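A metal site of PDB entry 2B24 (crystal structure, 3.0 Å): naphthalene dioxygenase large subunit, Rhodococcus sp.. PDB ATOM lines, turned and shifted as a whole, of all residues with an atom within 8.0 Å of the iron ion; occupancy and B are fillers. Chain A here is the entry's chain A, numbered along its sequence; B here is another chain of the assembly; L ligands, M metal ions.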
ATOM      1  N   ASN A 209      -8.399  -7.935  17.407  1.00  0.00           N
ATOM      2  CA  ASN A 209      -7.627  -6.708  17.225  1.00  0.00           C
ATOM      3  C   ASN A 209      -8.332  -5.442  17.685  1.00  0.00           C
ATOM      4  O   ASN A 209      -7.697  -4.558  18.254  1.00  0.00           O
ATOM      5  CB  ASN A 209      -7.190  -6.536  15.768  1.00  0.00           C
ATOM      6  CG  ASN A 209      -6.067  -5.540  15.603  1.00  0.00           C
ATOM      7  OD1 ASN A 209      -6.264  -4.442  15.096  1.00  0.00           O
ATOM      8  ND2 ASN A 209      -4.881  -5.909  16.046  1.00  0.00           N
ATOM      9  N   PHE A 210      -9.626  -5.351  17.432  1.00  0.00           N
ATOM     10  CA  PHE A 210     -10.379  -4.118  17.751  1.00  0.00           C
ATOM     11  C   PHE A 210     -10.863  -4.001  19.191  1.00  0.00           C
ATOM     12  O   PHE A 210     -10.989  -2.879  19.695  1.00  0.00           O
ATOM     13  CB  PHE A 210     -11.513  -3.873  16.755  1.00  0.00           C
ATOM     14  CG  PHE A 210     -11.096  -3.099  15.544  1.00  0.00           C
ATOM     15  CD1 PHE A 210     -10.255  -3.670  14.585  1.00  0.00           C
ATOM     16  CD2 PHE A 210     -11.528  -1.790  15.355  1.00  0.00           C
ATOM     17  CE1 PHE A 210      -9.866  -2.940  13.466  1.00  0.00           C
ATOM     18  CE2 PHE A 210     -11.144  -1.058  14.249  1.00  0.00           C
ATOM     19  CZ  PHE A 210     -10.309  -1.629  13.302  1.00  0.00           C
ATOM     20  N   ASP A 213      -6.757  -3.864  21.212  1.00  0.00           N
ATOM     21  CA  ASP A 213      -5.371  -3.879  20.769  1.00  0.00           C
ATOM     22  C   ASP A 213      -4.955  -2.538  20.246  1.00  0.00           C
ATOM     23  O   ASP A 213      -5.109  -2.257  19.057  1.00  0.00           O
ATOM     24  CB  ASP A 213      -5.116  -4.991  19.743  1.00  0.00           C
ATOM     25  CG  ASP A 213      -3.764  -5.649  19.915  1.00  0.00           C
ATOM     26  OD1 ASP A 213      -2.737  -4.970  19.710  1.00  0.00           O
ATOM     27  OD2 ASP A 213      -3.628  -6.853  20.251  1.00  0.00           O
ATOM     28  N   ALA A 214      -4.473  -1.690  21.153  1.00  0.00           N
ATOM     29  CA  ALA A 214      -3.844  -0.409  20.809  1.00  0.00           C
ATOM     30  C   ALA A 214      -2.355  -0.556  20.932  1.00  0.00           C
ATOM     31  O   ALA A 214      -1.606   0.183  20.315  1.00  0.00           O
ATOM     32  CB  ALA A 214      -4.331   0.686  21.694  1.00  0.00           C
ATOM     33  N   HIS A 216      -0.513  -2.757  19.531  1.00  0.00           N
ATOM     34  CA  HIS A 216       0.089  -3.081  18.224  1.00  0.00           C
ATOM     35  C   HIS A 216       0.401  -1.892  17.324  1.00  0.00           C
ATOM     36  O   HIS A 216       1.265  -1.982  16.485  1.00  0.00           O
ATOM     37  CB  HIS A 216      -0.779  -4.096  17.460  1.00  0.00           C
ATOM     38  CG  HIS A 216      -1.899  -3.483  16.674  1.00  0.00           C
ATOM     39  ND1 HIS A 216      -2.998  -2.897  17.272  1.00  0.00           N
ATOM     40  CD2 HIS A 216      -2.101  -3.385  15.347  1.00  0.00           C
ATOM     41  CE1 HIS A 216      -3.820  -2.469  16.347  1.00  0.00           C
ATOM     42  NE2 HIS A 216      -3.307  -2.745  15.160  1.00  0.00           N
ATOM     43  N   THR A 217      -0.303  -0.788  17.527  1.00  0.00           N
ATOM     44  CA  THR A 217      -0.052   0.440  16.768  1.00  0.00           C
ATOM     45  C   THR A 217       1.409   0.740  16.471  1.00  0.00           C
ATOM     46  O   THR A 217       1.712   1.295  15.437  1.00  0.00           O
ATOM     47  CB  THR A 217      -0.634   1.631  17.499  1.00  0.00           C
ATOM     48  OG1 THR A 217      -2.057   1.538  17.489  1.00  0.00           O
ATOM     49  CG2 THR A 217      -0.346   2.899  16.721  1.00  0.00           C
ATOM     50  N   MET A 218       2.326   0.372  17.363  1.00  0.00           N
ATOM     51  CA  MET A 218       3.700   0.867  17.269  1.00  0.00           C
ATOM     52  C   MET A 218       4.663   0.011  16.480  1.00  0.00           C
ATOM     53  O   MET A 218       5.584   0.538  15.920  1.00  0.00           O
ATOM     54  CB  MET A 218       4.295   1.163  18.647  1.00  0.00           C
ATOM     55  CG  MET A 218       3.730   0.318  19.762  1.00  0.00           C
ATOM     56  SD  MET A 218       3.570   1.285  21.207  1.00  0.00           S
ATOM     57  CE  MET A 218       5.380   1.590  21.493  1.00  0.00           C
ATOM     58  N   THR A 220       3.411  -2.805  14.159  1.00  0.00           N
ATOM     59  CA  THR A 220       2.800  -3.094  12.875  1.00  0.00           C
ATOM     60  C   THR A 220       2.500  -1.830  12.091  1.00  0.00           C
ATOM     61  O   THR A 220       2.727  -1.793  10.885  1.00  0.00           O
ATOM     62  CB  THR A 220       1.579  -4.044  13.011  1.00  0.00           C
ATOM     63  OG1 THR A 220       0.603  -3.725  12.029  1.00  0.00           O
ATOM     64  CG2 THR A 220       0.866  -3.798  14.262  1.00  0.00           C
ATOM     65  N   HIS A 221       2.045  -0.780  12.793  1.00  0.00           N
ATOM     66  CA  HIS A 221       1.818   0.530  12.181  1.00  0.00           C
ATOM     67  C   HIS A 221       2.976   1.499  12.417  1.00  0.00           C
ATOM     68  O   HIS A 221       2.791   2.717  12.513  1.00  0.00           O
ATOM     69  CB  HIS A 221       0.473   1.119  12.631  1.00  0.00           C
ATOM     70  CG  HIS A 221      -0.664   0.167  12.473  1.00  0.00           C
ATOM     71  ND1 HIS A 221      -1.031  -0.352  11.260  1.00  0.00           N
ATOM     72  CD2 HIS A 221      -1.492  -0.389  13.388  1.00  0.00           C
ATOM     73  CE1 HIS A 221      -2.055  -1.175  11.422  1.00  0.00           C
ATOM     74  NE2 HIS A 221      -2.358  -1.217  12.704  1.00  0.00           N
ATOM     75  N   PHE A 307     -11.645   6.942  14.783  1.00  0.00           N
ATOM     76  CA  PHE A 307     -10.258   7.375  14.907  1.00  0.00           C
ATOM     77  C   PHE A 307     -10.048   8.780  14.356  1.00  0.00           C
ATOM     78  O   PHE A 307     -10.533   9.103  13.278  1.00  0.00           O
ATOM     79  CB  PHE A 307      -9.321   6.440  14.136  1.00  0.00           C
ATOM     80  CG  PHE A 307      -9.435   4.982  14.501  1.00  0.00           C
ATOM     81  CD1 PHE A 307      -9.686   4.034  13.529  1.00  0.00           C
ATOM     82  CD2 PHE A 307      -9.268   4.570  15.805  1.00  0.00           C
ATOM     83  CE1 PHE A 307      -9.796   2.693  13.848  1.00  0.00           C
ATOM     84  CE2 PHE A 307      -9.374   3.220  16.135  1.00  0.00           C
ATOM     85  CZ  PHE A 307      -9.638   2.281  15.157  1.00  0.00           C
ATOM     86  N   THR A 361      -6.203   5.476   5.510  1.00  0.00           N
ATOM     87  CA  THR A 361      -5.706   4.791   6.702  1.00  0.00           C
ATOM     88  C   THR A 361      -6.292   3.396   6.866  1.00  0.00           C
ATOM     89  O   THR A 361      -5.557   2.440   6.995  1.00  0.00           O
ATOM     90  CB  THR A 361      -5.959   5.600   7.951  1.00  0.00           C
ATOM     91  OG1 THR A 361      -7.347   5.903   7.988  1.00  0.00           O
ATOM     92  CG2 THR A 361      -5.270   6.944   7.879  1.00  0.00           C
ATOM     93  N   PHE A 362      -7.616   3.276   6.861  1.00  0.00           N
ATOM     94  CA  PHE A 362      -8.250   1.979   7.013  1.00  0.00           C
ATOM     95  C   PHE A 362      -8.914   1.519   5.734  1.00  0.00           C
ATOM     96  O   PHE A 362      -8.838   2.203   4.749  1.00  0.00           O
ATOM     97  CB  PHE A 362      -9.165   1.960   8.253  1.00  0.00           C
ATOM     98  CG  PHE A 362      -8.405   1.749   9.522  1.00  0.00           C
ATOM     99  CD1 PHE A 362      -7.541   2.730   9.987  1.00  0.00           C
ATOM    100  CD2 PHE A 362      -8.472   0.568  10.200  1.00  0.00           C
ATOM    101  CE1 PHE A 362      -6.780   2.528  11.124  1.00  0.00           C
ATOM    102  CE2 PHE A 362      -7.722   0.387  11.339  1.00  0.00           C
ATOM    103  CZ  PHE A 362      -6.875   1.376  11.789  1.00  0.00           C
ATOM    104  N   GLY A 367      -3.208   2.558   4.717  1.00  0.00           N
ATOM    105  CA  GLY A 367      -1.817   2.370   5.102  1.00  0.00           C
ATOM    106  C   GLY A 367      -1.719   1.647   6.431  1.00  0.00           C
ATOM    107  O   GLY A 367      -0.703   1.065   6.758  1.00  0.00           O
ATOM    108  N   PHE A 368      -2.793   1.717   7.207  1.00  0.00           N
ATOM    109  CA  PHE A 368      -2.867   1.026   8.485  1.00  0.00           C
ATOM    110  C   PHE A 368      -3.412  -0.390   8.253  1.00  0.00           C
ATOM    111  O   PHE A 368      -2.735  -1.376   8.529  1.00  0.00           O
ATOM    112  CB  PHE A 368      -3.790   1.767   9.452  1.00  0.00           C
ATOM    113  CG  PHE A 368      -3.154   2.932  10.147  1.00  0.00           C
ATOM    114  CD1 PHE A 368      -3.047   4.179   9.533  1.00  0.00           C
ATOM    115  CD2 PHE A 368      -2.731   2.827  11.459  1.00  0.00           C
ATOM    116  CE1 PHE A 368      -2.501   5.279  10.195  1.00  0.00           C
ATOM    117  CE2 PHE A 368      -2.181   3.918  12.131  1.00  0.00           C
ATOM    118  CZ  PHE A 368      -2.059   5.144  11.502  1.00  0.00           C
ATOM    119  N   GLU A 369      -4.633  -0.499   7.737  1.00  0.00           N
ATOM    120  CA  GLU A 369      -5.303  -1.772   7.696  1.00  0.00           C
ATOM    121  C   GLU A 369      -4.673  -2.800   6.735  1.00  0.00           C
ATOM    122  O   GLU A 369      -4.930  -4.000   6.853  1.00  0.00           O
ATOM    123  CB  GLU A 369      -6.790  -1.580   7.394  1.00  0.00           C
ATOM    124  CG  GLU A 369      -7.626  -2.851   7.422  1.00  0.00           C
ATOM    125  CD  GLU A 369      -8.974  -2.666   8.084  1.00  0.00           C
ATOM    126  OE1 GLU A 369      -9.921  -2.231   7.405  1.00  0.00           O
ATOM    127  OE2 GLU A 369      -9.080  -2.953   9.273  1.00  0.00           O
ATOM    128  N   GLN A 370      -3.861  -2.358   5.782  1.00  0.00           N
ATOM    129  CA  GLN A 370      -3.241  -3.331   4.875  1.00  0.00           C
ATOM    130  C   GLN A 370      -2.145  -4.154   5.559  1.00  0.00           C
ATOM    131  O   GLN A 370      -1.884  -5.273   5.173  1.00  0.00           O
ATOM    132  CB  GLN A 370      -2.736  -2.661   3.594  1.00  0.00           C
ATOM    133  CG  GLN A 370      -1.484  -1.836   3.771  1.00  0.00           C
ATOM    134  CD  GLN A 370      -1.044  -1.155   2.516  1.00  0.00           C
ATOM    135  OE1 GLN A 370       0.103  -1.272   2.127  1.00  0.00           O
ATOM    136  NE2 GLN A 370      -1.935  -0.424   1.885  1.00  0.00           N
ATOM    137  N   ASP A 371      -1.525  -3.583   6.597  1.00  0.00           N
ATOM    138  CA  ASP A 371      -0.550  -4.276   7.429  1.00  0.00           C
ATOM    139  C   ASP A 371      -1.238  -5.141   8.456  1.00  0.00           C
ATOM    140  O   ASP A 371      -0.691  -6.140   8.863  1.00  0.00           O
ATOM    141  CB  ASP A 371       0.312  -3.273   8.176  1.00  0.00           C
ATOM    142  CG  ASP A 371       1.260  -2.551   7.282  1.00  0.00           C
ATOM    143  OD1 ASP A 371       1.445  -2.981   6.147  1.00  0.00           O
ATOM    144  OD2 ASP A 371       1.883  -1.535   7.637  1.00  0.00           O
ATOM    145  N   ASP A 372      -2.424  -4.730   8.900  1.00  0.00           N
ATOM    146  CA  ASP A 372      -3.242  -5.571   9.772  1.00  0.00           C
ATOM    147  C   ASP A 372      -3.644  -6.844   9.044  1.00  0.00           C
ATOM    148  O   ASP A 372      -3.567  -7.911   9.598  1.00  0.00           O
ATOM    149  CB  ASP A 372      -4.454  -4.807  10.249  1.00  0.00           C
ATOM    150  CG  ASP A 372      -4.129  -3.723  11.265  1.00  0.00           C
ATOM    151  OD1 ASP A 372      -3.167  -3.868  12.052  1.00  0.00           O
ATOM    152  OD2 ASP A 372      -4.818  -2.703  11.404  1.00  0.00           O
ATOM    153  N   ALA A 373      -4.034  -6.744   7.785  1.00  0.00           N
ATOM    154  CA  ALA A 373      -4.469  -7.910   7.028  1.00  0.00           C
ATOM    155  C   ALA A 373      -3.333  -8.855   6.686  1.00  0.00           C
ATOM    156  O   ALA A 373      -3.576  -9.985   6.314  1.00  0.00           O
ATOM    157  CB  ALA A 373      -5.151  -7.476   5.761  1.00  0.00           C
ATOM    158  N   ASN A 375      -0.741  -9.370   8.884  1.00  0.00           N
ATOM    159  CA  ASN A 375      -0.439 -10.003  10.153  1.00  0.00           C
ATOM    160  C   ASN A 375      -1.446 -11.091  10.496  1.00  0.00           C
ATOM    161  O   ASN A 375      -1.048 -12.199  10.833  1.00  0.00           O
ATOM    162  CB  ASN A 375      -0.383  -8.950  11.229  1.00  0.00           C
ATOM    163  CG  ASN A 375       0.805  -8.044  11.066  1.00  0.00           C
ATOM    164  OD1 ASN A 375       1.667  -8.233  10.226  1.00  0.00           O
ATOM    165  ND2 ASN A 375       0.848  -7.011  11.900  1.00  0.00           N
ATOM    166  N   TRP A 376      -2.727 -10.791  10.348  1.00  0.00           N
ATOM    167  CA  TRP A 376      -3.773 -11.760  10.566  1.00  0.00           C
ATOM    168  C   TRP A 376      -3.658 -12.947   9.648  1.00  0.00           C
ATOM    169  O   TRP A 376      -3.864 -14.059  10.095  1.00  0.00           O
ATOM    170  CB  TRP A 376      -5.156 -11.143  10.399  1.00  0.00           C
ATOM    171  CG  TRP A 376      -5.371  -9.943  11.259  1.00  0.00           C
ATOM    172  CD1 TRP A 376      -4.743  -9.653  12.428  1.00  0.00           C
ATOM    173  CD2 TRP A 376      -6.257  -8.861  10.996  1.00  0.00           C
ATOM    174  NE1 TRP A 376      -5.188  -8.449  12.916  1.00  0.00           N
ATOM    175  CE2 TRP A 376      -6.129  -7.948  12.066  1.00  0.00           C
ATOM    176  CE3 TRP A 376      -7.163  -8.573   9.977  1.00  0.00           C
ATOM    177  CZ2 TRP A 376      -6.867  -6.775  12.135  1.00  0.00           C
ATOM    178  CZ3 TRP A 376      -7.891  -7.410  10.043  1.00  0.00           C
ATOM    179  CH2 TRP A 376      -7.736  -6.525  11.126  1.00  0.00           C
ATOM    180  N   TYR B 110       3.811  -7.959  14.353  1.00  0.00           N
ATOM    181  CA  TYR B 110       2.562  -7.592  15.012  1.00  0.00           C
ATOM    182  C   TYR B 110       2.814  -6.591  16.142  1.00  0.00           C
ATOM    183  O   TYR B 110       2.519  -5.437  15.974  1.00  0.00           O
ATOM    184  CB  TYR B 110       1.808  -8.846  15.471  1.00  0.00           C
ATOM    185  CG  TYR B 110       0.280  -8.774  15.544  1.00  0.00           C
ATOM    186  CD1 TYR B 110      -0.450  -9.934  15.801  1.00  0.00           C
ATOM    187  CD2 TYR B 110      -0.420  -7.588  15.390  1.00  0.00           C
ATOM    188  CE1 TYR B 110      -1.829  -9.927  15.894  1.00  0.00           C
ATOM    189  CE2 TYR B 110      -1.831  -7.572  15.485  1.00  0.00           C
ATOM    190  CZ  TYR B 110      -2.532  -8.762  15.732  1.00  0.00           C
ATOM    191  OH  TYR B 110      -3.904  -8.826  15.818  1.00  0.00           O
HETATM  192  N1  LIG L   1      -6.889  -0.027  17.963  1.00  0.00           N
HETATM  193  C1  LIG L   1      -7.376  -0.585  16.803  1.00  0.00           C
HETATM  194  C2  LIG L   1      -7.182   0.251  15.680  1.00  0.00           C
HETATM  195  C3  LIG L   1      -6.109   2.565  15.568  1.00  0.00           C
HETATM  196  C4  LIG L   1      -5.497   3.537  16.366  1.00  0.00           C
HETATM  197  C5  LIG L   1      -5.350   3.341  17.747  1.00  0.00           C
HETATM  198  C6  LIG L   1      -5.789   2.180  18.393  1.00  0.00           C
HETATM  199  C7  LIG L   1      -6.405   1.159  17.611  1.00  0.00           C
HETATM  200  C8  LIG L   1      -6.564   1.362  16.203  1.00  0.00           C
HETATM  201 FE    FE M   1      -4.129  -1.800  13.307  1.00  0.00          FE
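O of Asp 213 lies within hydrogen-bond range of N1 of the ligand, at 3.1 Å.
ND1 of His 221 sits close to O of Phe 368 (3.4 Å). A ring nitrogen (NE2) of His 216 lies close to the side-chain amide oxygen (OD1) of Asn 209. ND1 of His 216 sits at hydrogen-bond distance from O of Asp 213 (2.8 Å). The side-chain amide nitrogen of Asn 209 is in hydrogen-bond range of the side-chain hydroxyl of Tyr 110 of chain B (3.1 Å).
Merely in contact with the iron ion: Asn 209.
The iron ion is bound by a ring nitrogen (NE2) of His 221 (2.0 Å), the side-chain carboxylate (OD2) of Asp 372 (2.2 Å) and a ring nitrogen (NE2) of His 216 (2.2 Å). Slightly farther from the iron ion lies OD1 of Asp 372 (2.6 Å).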
